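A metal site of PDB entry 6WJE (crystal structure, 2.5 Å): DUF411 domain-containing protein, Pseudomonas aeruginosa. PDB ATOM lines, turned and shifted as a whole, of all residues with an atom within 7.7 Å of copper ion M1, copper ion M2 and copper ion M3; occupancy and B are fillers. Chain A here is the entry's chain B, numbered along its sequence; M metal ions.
The side-chain sulfur of Cys 16 forms a disulfide with the side-chain sulfur of Cys 13 (2.1 Å). O of Pro 95 lies within hydrogen-bond range of ND1 of His 67 (2.6 Å). The side-chain sulfur of Cys 13 sits close to the side-chain sulfur of Cys 15, 3.3 Å away. A ring nitrogen (NE2) of His 55 is in hydrogen-bond range of the backbone carbonyl oxygen (O) of Gly 66, at 2.7 Å.
Copper ion M1 is bound by SG of Cys 15 (2.4 Å), SD of Met 90 (2.4 Å) and SD of Met 97 (2.5 Å).
Of the 29 residues printed, 3 come within 4 Å of copper ion M1.
The nearest printed residue that does not touch copper ion M2 is Cys 13 (4.1 Å).
Copper ion M3 is bound by a ring nitrogen (ND1) of His 55 (2.1 Å), the side-chain sulfur of Cys 54 (2.3 Å) and the side-chain sulfur of Cys 16 (2.3 Å). Copper ion M3 has three donor atoms within binding distance.
Copper ion M2 is bound by a ring nitrogen (NE2) of His 67, the side-chain sulfur of Cys 15 and the side-chain sulfur of Cys 54.
Residues that only touch copper ion M3: Cys 13. Of the 29 residues printed, 5 come within 4 Å of copper ion M3. The nearest printed residue that does not touch copper ion M3 is Cys 15 (4.3 Å).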
ATOM      1  N   VAL A   7      10.624  24.673  -1.795  1.00  0.00           N
ATOM      2  CA  VAL A   7      11.583  23.922  -0.988  1.00  0.00           C
ATOM      3  C   VAL A   7      13.017  24.369  -1.303  1.00  0.00           C
ATOM      4  O   VAL A   7      13.395  24.457  -2.477  1.00  0.00           O
ATOM      5  CB  VAL A   7      11.449  22.398  -1.195  1.00  0.00           C
ATOM      6  CG1 VAL A   7      12.463  21.680  -0.343  1.00  0.00           C
ATOM      7  CG2 VAL A   7      10.027  21.916  -0.855  1.00  0.00           C
ATOM      8  N   HIS A   8      13.805  24.646  -0.257  1.00  0.00           N
ATOM      9  CA  HIS A   8      15.210  25.024  -0.400  1.00  0.00           C
ATOM     10  C   HIS A   8      16.115  23.982   0.250  1.00  0.00           C
ATOM     11  O   HIS A   8      15.850  23.527   1.357  1.00  0.00           O
ATOM     12  CB  HIS A   8      15.452  26.397   0.208  1.00  0.00           C
ATOM     13  CG  HIS A   8      14.648  27.486  -0.435  1.00  0.00           C
ATOM     14  ND1 HIS A   8      15.211  28.458  -1.233  1.00  0.00           N
ATOM     15  CD2 HIS A   8      13.320  27.768  -0.383  1.00  0.00           C
ATOM     16  CE1 HIS A   8      14.275  29.288  -1.665  1.00  0.00           C
ATOM     17  NE2 HIS A   8      13.113  28.897  -1.162  1.00  0.00           N
ATOM     18  N   ARG A   9      17.206  23.628  -0.442  1.00  0.00           N
ATOM     19  CA  ARG A   9      18.038  22.510  -0.002  1.00  0.00           C
ATOM     20  C   ARG A   9      19.396  22.528  -0.692  1.00  0.00           C
ATOM     21  O   ARG A   9      19.616  23.256  -1.665  1.00  0.00           O
ATOM     22  CB  ARG A   9      17.377  21.186  -0.316  1.00  0.00           C
ATOM     23  CG  ARG A   9      17.121  21.095  -1.764  1.00  0.00           C
ATOM     24  CD  ARG A   9      17.094  19.687  -2.245  1.00  0.00           C
ATOM     25  NE  ARG A   9      16.797  19.685  -3.675  1.00  0.00           N
ATOM     26  CZ  ARG A   9      17.601  19.194  -4.602  1.00  0.00           C
ATOM     27  NH1 ARG A   9      18.774  18.648  -4.275  1.00  0.00           N
ATOM     28  NH2 ARG A   9      17.229  19.251  -5.866  1.00  0.00           N
ATOM     29  N   ASP A  10      20.308  21.719  -0.160  1.00  0.00           N
ATOM     30  CA  ASP A  10      21.638  21.539  -0.734  1.00  0.00           C
ATOM     31  C   ASP A  10      21.587  20.612  -1.954  1.00  0.00           C
ATOM     32  O   ASP A  10      20.736  19.730  -2.053  1.00  0.00           O
ATOM     33  CB  ASP A  10      22.595  20.969   0.300  1.00  0.00           C
ATOM     34  CG  ASP A  10      24.030  20.897  -0.221  1.00  0.00           C
ATOM     35  OD1 ASP A  10      24.725  21.929  -0.144  1.00  0.00           O
ATOM     36  OD2 ASP A  10      24.444  19.809  -0.700  1.00  0.00           O
ATOM     37  N   CYS A  13      22.037  16.687  -1.177  1.00  0.00           N
ATOM     38  CA  CYS A  13      21.079  16.234  -0.106  1.00  0.00           C
ATOM     39  C   CYS A  13      20.033  15.330  -0.744  1.00  0.00           C
ATOM     40  O   CYS A  13      19.043  15.866  -1.273  1.00  0.00           O
ATOM     41  CB  CYS A  13      20.244  17.351   0.553  1.00  0.00           C
ATOM     42  SG  CYS A  13      19.202  16.795   1.948  1.00  0.00           S
ATOM     43  N   GLY A  14      20.233  14.004  -0.707  1.00  0.00           N
ATOM     44  CA  GLY A  14      19.247  13.147  -1.300  1.00  0.00           C
ATOM     45  C   GLY A  14      18.077  12.832  -0.385  1.00  0.00           C
ATOM     46  O   GLY A  14      16.972  12.637  -0.917  1.00  0.00           O
ATOM     47  N   CYS A  15      18.277  12.662   0.930  1.00  0.00           N
ATOM     48  CA  CYS A  15      17.133  12.649   1.835  1.00  0.00           C
ATOM     49  C   CYS A  15      16.150  13.767   1.518  1.00  0.00           C
ATOM     50  O   CYS A  15      14.938  13.521   1.484  1.00  0.00           O
ATOM     51  CB  CYS A  15      17.583  12.660   3.307  1.00  0.00           C
ATOM     52  SG  CYS A  15      18.447  14.175   3.818  1.00  0.00           S
ATOM     53  N   CYS A  16      16.645  14.982   1.277  1.00  0.00           N
ATOM     54  CA  CYS A  16      15.728  16.059   0.900  1.00  0.00           C
ATOM     55  C   CYS A  16      15.015  15.776  -0.428  1.00  0.00           C
ATOM     56  O   CYS A  16      13.805  16.003  -0.550  1.00  0.00           O
ATOM     57  CB  CYS A  16      16.453  17.409   0.814  1.00  0.00           C
ATOM     58  SG  CYS A  16      17.411  17.867   2.218  1.00  0.00           S
ATOM     59  N   LYS A  17      15.756  15.276  -1.427  1.00  0.00           N
ATOM     60  CA  LYS A  17      15.135  15.004  -2.721  1.00  0.00           C
ATOM     61  C   LYS A  17      14.073  13.913  -2.619  1.00  0.00           C
ATOM     62  O   LYS A  17      13.031  14.010  -3.272  1.00  0.00           O
ATOM     63  CB  LYS A  17      16.193  14.558  -3.756  1.00  0.00           C
ATOM     64  CG  LYS A  17      17.192  15.607  -4.189  1.00  0.00           C
ATOM     65  CD  LYS A  17      18.305  15.043  -5.085  1.00  0.00           C
ATOM     66  N   ASP A  18      14.315  12.937  -1.747  1.00  0.00           N
ATOM     67  CA  ASP A  18      13.344  11.842  -1.499  1.00  0.00           C
ATOM     68  C   ASP A  18      12.064  12.462  -0.902  1.00  0.00           C
ATOM     69  O   ASP A  18      10.965  12.100  -1.363  1.00  0.00           O
ATOM     70  CB  ASP A  18      13.937  10.766  -0.586  1.00  0.00           C
ATOM     71  CG  ASP A  18      12.978   9.628  -0.273  1.00  0.00           C
ATOM     72  OD1 ASP A  18      11.942   9.537  -0.971  1.00  0.00           O
ATOM     73  OD2 ASP A  18      13.267   8.855   0.655  1.00  0.00           O
ATOM     74  N   TRP A  19      12.224  13.356   0.076  1.00  0.00           N
ATOM     75  CA  TRP A  19      11.108  14.042   0.699  1.00  0.00           C
ATOM     76  C   TRP A  19      10.274  14.798  -0.317  1.00  0.00           C
ATOM     77  O   TRP A  19       9.032  14.750  -0.260  1.00  0.00           O
ATOM     78  CB  TRP A  19      11.659  15.007   1.751  1.00  0.00           C
ATOM     79  CG  TRP A  19      10.632  15.722   2.576  1.00  0.00           C
ATOM     80  CD1 TRP A  19       9.881  15.192   3.587  1.00  0.00           C
ATOM     81  CD2 TRP A  19      10.239  17.094   2.459  1.00  0.00           C
ATOM     82  NE1 TRP A  19       9.055  16.154   4.123  1.00  0.00           N
ATOM     83  CE2 TRP A  19       9.247  17.329   3.445  1.00  0.00           C
ATOM     84  CE3 TRP A  19      10.626  18.151   1.614  1.00  0.00           C
ATOM     85  CZ2 TRP A  19       8.647  18.580   3.621  1.00  0.00           C
ATOM     86  CZ3 TRP A  19      10.041  19.398   1.798  1.00  0.00           C
ATOM     87  CH2 TRP A  19       9.059  19.600   2.799  1.00  0.00           C
ATOM     88  N   MET A  38      21.929  28.240   3.119  1.00  0.00           N
ATOM     89  CA  MET A  38      20.676  27.854   3.775  1.00  0.00           C
ATOM     90  C   MET A  38      20.382  28.608   5.063  1.00  0.00           C
ATOM     91  O   MET A  38      19.208  28.726   5.435  1.00  0.00           O
ATOM     92  CB  MET A  38      20.749  26.363   4.147  1.00  0.00           C
ATOM     93  CG  MET A  38      20.671  25.348   3.035  1.00  0.00           C
ATOM     94  SD  MET A  38      19.031  25.314   2.342  1.00  0.00           S
ATOM     95  CE  MET A  38      17.998  25.276   3.827  1.00  0.00           C
ATOM     96  N   LYS A  42      16.718  30.205   6.396  1.00  0.00           N
ATOM     97  CA  LYS A  42      16.083  29.905   7.678  1.00  0.00           C
ATOM     98  C   LYS A  42      15.842  31.193   8.445  1.00  0.00           C
ATOM     99  O   LYS A  42      14.812  31.349   9.121  1.00  0.00           O
ATOM    100  CB  LYS A  42      16.925  28.920   8.480  1.00  0.00           C
ATOM    101  CG  LYS A  42      17.134  27.579   7.755  1.00  0.00           C
ATOM    102  CD  LYS A  42      17.726  26.482   8.656  1.00  0.00           C
ATOM    103  CE  LYS A  42      18.295  25.289   7.856  1.00  0.00           C
ATOM    104  NZ  LYS A  42      17.270  24.560   7.029  1.00  0.00           N
ATOM    105  N   SER A  53      17.087  21.958  10.245  1.00  0.00           N
ATOM    106  CA  SER A  53      17.134  20.625   9.686  1.00  0.00           C
ATOM    107  C   SER A  53      17.788  20.743   8.317  1.00  0.00           C
ATOM    108  O   SER A  53      18.438  21.754   8.021  1.00  0.00           O
ATOM    109  CB  SER A  53      15.720  20.030   9.621  1.00  0.00           C
ATOM    110  OG  SER A  53      15.834  18.641   9.514  1.00  0.00           O
ATOM    111  N   CYS A  54      17.696  19.697   7.502  1.00  0.00           N
ATOM    112  CA  CYS A  54      18.418  19.689   6.238  1.00  0.00           C
ATOM    113  C   CYS A  54      17.799  20.585   5.165  1.00  0.00           C
ATOM    114  O   CYS A  54      18.468  20.849   4.170  1.00  0.00           O
ATOM    115  CB  CYS A  54      18.578  18.259   5.717  1.00  0.00           C
ATOM    116  SG  CYS A  54      17.166  17.280   6.129  1.00  0.00           S
ATOM    117  N   HIS A  55      16.544  20.953   5.285  1.00  0.00           N
ATOM    118  CA  HIS A  55      15.884  21.663   4.198  1.00  0.00           C
ATOM    119  C   HIS A  55      14.806  22.531   4.804  1.00  0.00           C
ATOM    120  O   HIS A  55      14.380  22.320   5.931  1.00  0.00           O
ATOM    121  CB  HIS A  55      15.292  20.724   3.136  1.00  0.00           C
ATOM    122  CG  HIS A  55      14.162  19.864   3.649  1.00  0.00           C
ATOM    123  ND1 HIS A  55      14.292  18.499   3.881  1.00  0.00           N
ATOM    124  CD2 HIS A  55      12.874  20.164   3.921  1.00  0.00           C
ATOM    125  CE1 HIS A  55      13.140  18.022   4.321  1.00  0.00           C
ATOM    126  NE2 HIS A  55      12.265  19.002   4.356  1.00  0.00           N
ATOM    127  N   THR A  56      14.388  23.545   4.033  1.00  0.00           N
ATOM    128  CA  THR A  56      13.391  24.482   4.498  1.00  0.00           C
ATOM    129  C   THR A  56      12.359  24.724   3.408  1.00  0.00           C
ATOM    130  O   THR A  56      12.704  25.207   2.330  1.00  0.00           O
ATOM    131  CB  THR A  56      14.050  25.799   4.934  1.00  0.00           C
ATOM    132  OG1 THR A  56      15.105  25.510   5.880  1.00  0.00           O
ATOM    133  CG2 THR A  56      13.036  26.726   5.597  1.00  0.00           C
ATOM    134  N   GLU A  65      10.073  22.902   8.340  1.00  0.00           N
ATOM    135  CA  GLU A  65      11.493  22.632   8.517  1.00  0.00           C
ATOM    136  C   GLU A  65      11.716  21.124   8.682  1.00  0.00           C
ATOM    137  O   GLU A  65      11.197  20.511   9.626  1.00  0.00           O
ATOM    138  CB  GLU A  65      12.040  23.421   9.703  1.00  0.00           C
ATOM    139  CG  GLU A  65      13.529  23.299   9.925  1.00  0.00           C
ATOM    140  CD  GLU A  65      14.319  23.978   8.832  1.00  0.00           C
ATOM    141  OE1 GLU A  65      13.693  24.732   8.041  1.00  0.00           O
ATOM    142  OE2 GLU A  65      15.549  23.774   8.757  1.00  0.00           O
ATOM    143  N   GLY A  66      12.446  20.521   7.746  1.00  0.00           N
ATOM    144  CA  GLY A  66      12.784  19.120   7.850  1.00  0.00           C
ATOM    145  C   GLY A  66      11.698  18.173   7.337  1.00  0.00           C
ATOM    146  O   GLY A  66      10.795  18.541   6.586  1.00  0.00           O
ATOM    147  N   HIS A  67      11.808  16.917   7.761  1.00  0.00           N
ATOM    148  CA  HIS A  67      11.049  15.811   7.185  1.00  0.00           C
ATOM    149  C   HIS A  67       9.677  15.690   7.824  1.00  0.00           C
ATOM    150  O   HIS A  67       9.307  14.675   8.434  1.00  0.00           O
ATOM    151  CB  HIS A  67      11.855  14.516   7.301  1.00  0.00           C
ATOM    152  CG  HIS A  67      13.059  14.514   6.413  1.00  0.00           C
ATOM    153  ND1 HIS A  67      13.040  13.947   5.158  1.00  0.00           N
ATOM    154  CD2 HIS A  67      14.271  15.089   6.558  1.00  0.00           C
ATOM    155  CE1 HIS A  67      14.226  14.132   4.584  1.00  0.00           C
ATOM    156  NE2 HIS A  67      14.985  14.832   5.420  1.00  0.00           N
ATOM    157  N   GLY A  89      16.715  18.036  13.157  1.00  0.00           N
ATOM    158  CA  GLY A  89      17.651  16.980  12.844  1.00  0.00           C
ATOM    159  C   GLY A  89      17.171  16.159  11.661  1.00  0.00           C
ATOM    160  O   GLY A  89      16.510  16.660  10.755  1.00  0.00           O
ATOM    161  N   MET A  90      17.527  14.862  11.671  1.00  0.00           N
ATOM    162  CA  MET A  90      17.186  13.949  10.573  1.00  0.00           C
ATOM    163  C   MET A  90      16.866  12.580  11.151  1.00  0.00           C
ATOM    164  O   MET A  90      17.661  11.640  11.044  1.00  0.00           O
ATOM    165  CB  MET A  90      18.341  13.850   9.571  1.00  0.00           C
ATOM    166  CG  MET A  90      18.294  14.797   8.410  1.00  0.00           C
ATOM    167  SD  MET A  90      19.779  14.558   7.366  1.00  0.00           S
ATOM    168  CE  MET A  90      20.951  14.045   8.601  1.00  0.00           C
ATOM    169  N   PRO A  91      15.714  12.432  11.805  1.00  0.00           N
ATOM    170  CA  PRO A  91      15.376  11.132  12.395  1.00  0.00           C
ATOM    171  C   PRO A  91      15.097  10.054  11.346  1.00  0.00           C
ATOM    172  O   PRO A  91      14.343  10.273  10.394  1.00  0.00           O
ATOM    173  CB  PRO A  91      14.121  11.436  13.236  1.00  0.00           C
ATOM    174  CG  PRO A  91      13.568  12.674  12.683  1.00  0.00           C
ATOM    175  CD  PRO A  91      14.735  13.468  12.145  1.00  0.00           C
ATOM    176  N   VAL A  92      15.717   8.882  11.534  1.00  0.00           N
ATOM    177  CA  VAL A  92      15.455   7.768  10.632  1.00  0.00           C
ATOM    178  C   VAL A  92      13.991   7.332  10.770  1.00  0.00           C
ATOM    179  O   VAL A  92      13.449   7.269  11.887  1.00  0.00           O
ATOM    180  CB  VAL A  92      16.423   6.610  10.927  1.00  0.00           C
ATOM    181  CG1 VAL A  92      15.873   5.294  10.407  1.00  0.00           C
ATOM    182  CG2 VAL A  92      17.799   6.860  10.302  1.00  0.00           C
ATOM    183  N   SER A  94      11.420   9.011   9.338  1.00  0.00           N
ATOM    184  CA  SER A  94      10.601  10.121   8.864  1.00  0.00           C
ATOM    185  C   SER A  94      10.601  10.154   7.328  1.00  0.00           C
ATOM    186  O   SER A  94      11.572   9.723   6.713  1.00  0.00           O
ATOM    187  CB  SER A  94      11.109  11.443   9.454  1.00  0.00           C
ATOM    188  OG  SER A  94      12.414  11.765   8.996  1.00  0.00           O
ATOM    189  N   PRO A  95       9.565  10.722   6.699  1.00  0.00           N
ATOM    190  CA  PRO A  95       9.465  10.644   5.231  1.00  0.00           C
ATOM    191  C   PRO A  95      10.631  11.332   4.536  1.00  0.00           C
ATOM    192  O   PRO A  95      10.948  12.498   4.807  1.00  0.00           O
ATOM    193  CB  PRO A  95       8.127  11.326   4.923  1.00  0.00           C
ATOM    194  CG  PRO A  95       7.403  11.336   6.177  1.00  0.00           C
ATOM    195  CD  PRO A  95       8.386  11.368   7.289  1.00  0.00           C
ATOM    196  N   GLY A  96      11.244  10.613   3.599  1.00  0.00           N
ATOM    197  CA  GLY A  96      12.468  11.006   2.940  1.00  0.00           C
ATOM    198  C   GLY A  96      13.720  10.587   3.677  1.00  0.00           C
ATOM    199  O   GLY A  96      14.815  10.692   3.111  1.00  0.00           O
ATOM    200  N   MET A  97      13.599  10.100   4.926  1.00  0.00           N
ATOM    201  CA  MET A  97      14.692   9.570   5.733  1.00  0.00           C
ATOM    202  C   MET A  97      14.436   8.122   6.155  1.00  0.00           C
ATOM    203  O   MET A  97      15.025   7.657   7.132  1.00  0.00           O
ATOM    204  CB  MET A  97      14.890  10.405   7.005  1.00  0.00           C
ATOM    205  CG  MET A  97      15.835  11.584   6.885  1.00  0.00           C
ATOM    206  SD  MET A  97      17.464  10.984   6.426  1.00  0.00           S
ATOM    207  CE  MET A  97      18.065  10.373   7.999  1.00  0.00           C
ATOM    208  N   MET A  99      14.600   4.150   6.213  1.00  0.00           N
ATOM    209  CA  MET A  99      15.670   3.242   5.911  1.00  0.00           C
ATOM    210  C   MET A  99      15.296   1.917   6.567  1.00  0.00           C
ATOM    211  O   MET A  99      15.896   1.450   7.531  1.00  0.00           O
ATOM    212  CB  MET A  99      17.021   3.795   6.395  1.00  0.00           C
ATOM    213  CG  MET A  99      17.446   5.066   5.692  1.00  0.00           C
ATOM    214  SD  MET A  99      18.921   5.828   6.403  1.00  0.00           S
ATOM    215  CE  MET A  99      19.000   7.341   5.469  1.00  0.00           C
HETATM  216 CU    CU M   1      18.950  12.887   5.802  1.00  0.00          CU
HETATM  217 CU    CU M   2      16.964  15.302   5.019  1.00  0.00          CU
HETATM  218 CU    CU M   3      16.231  17.813   4.151  1.00  0.00          CU
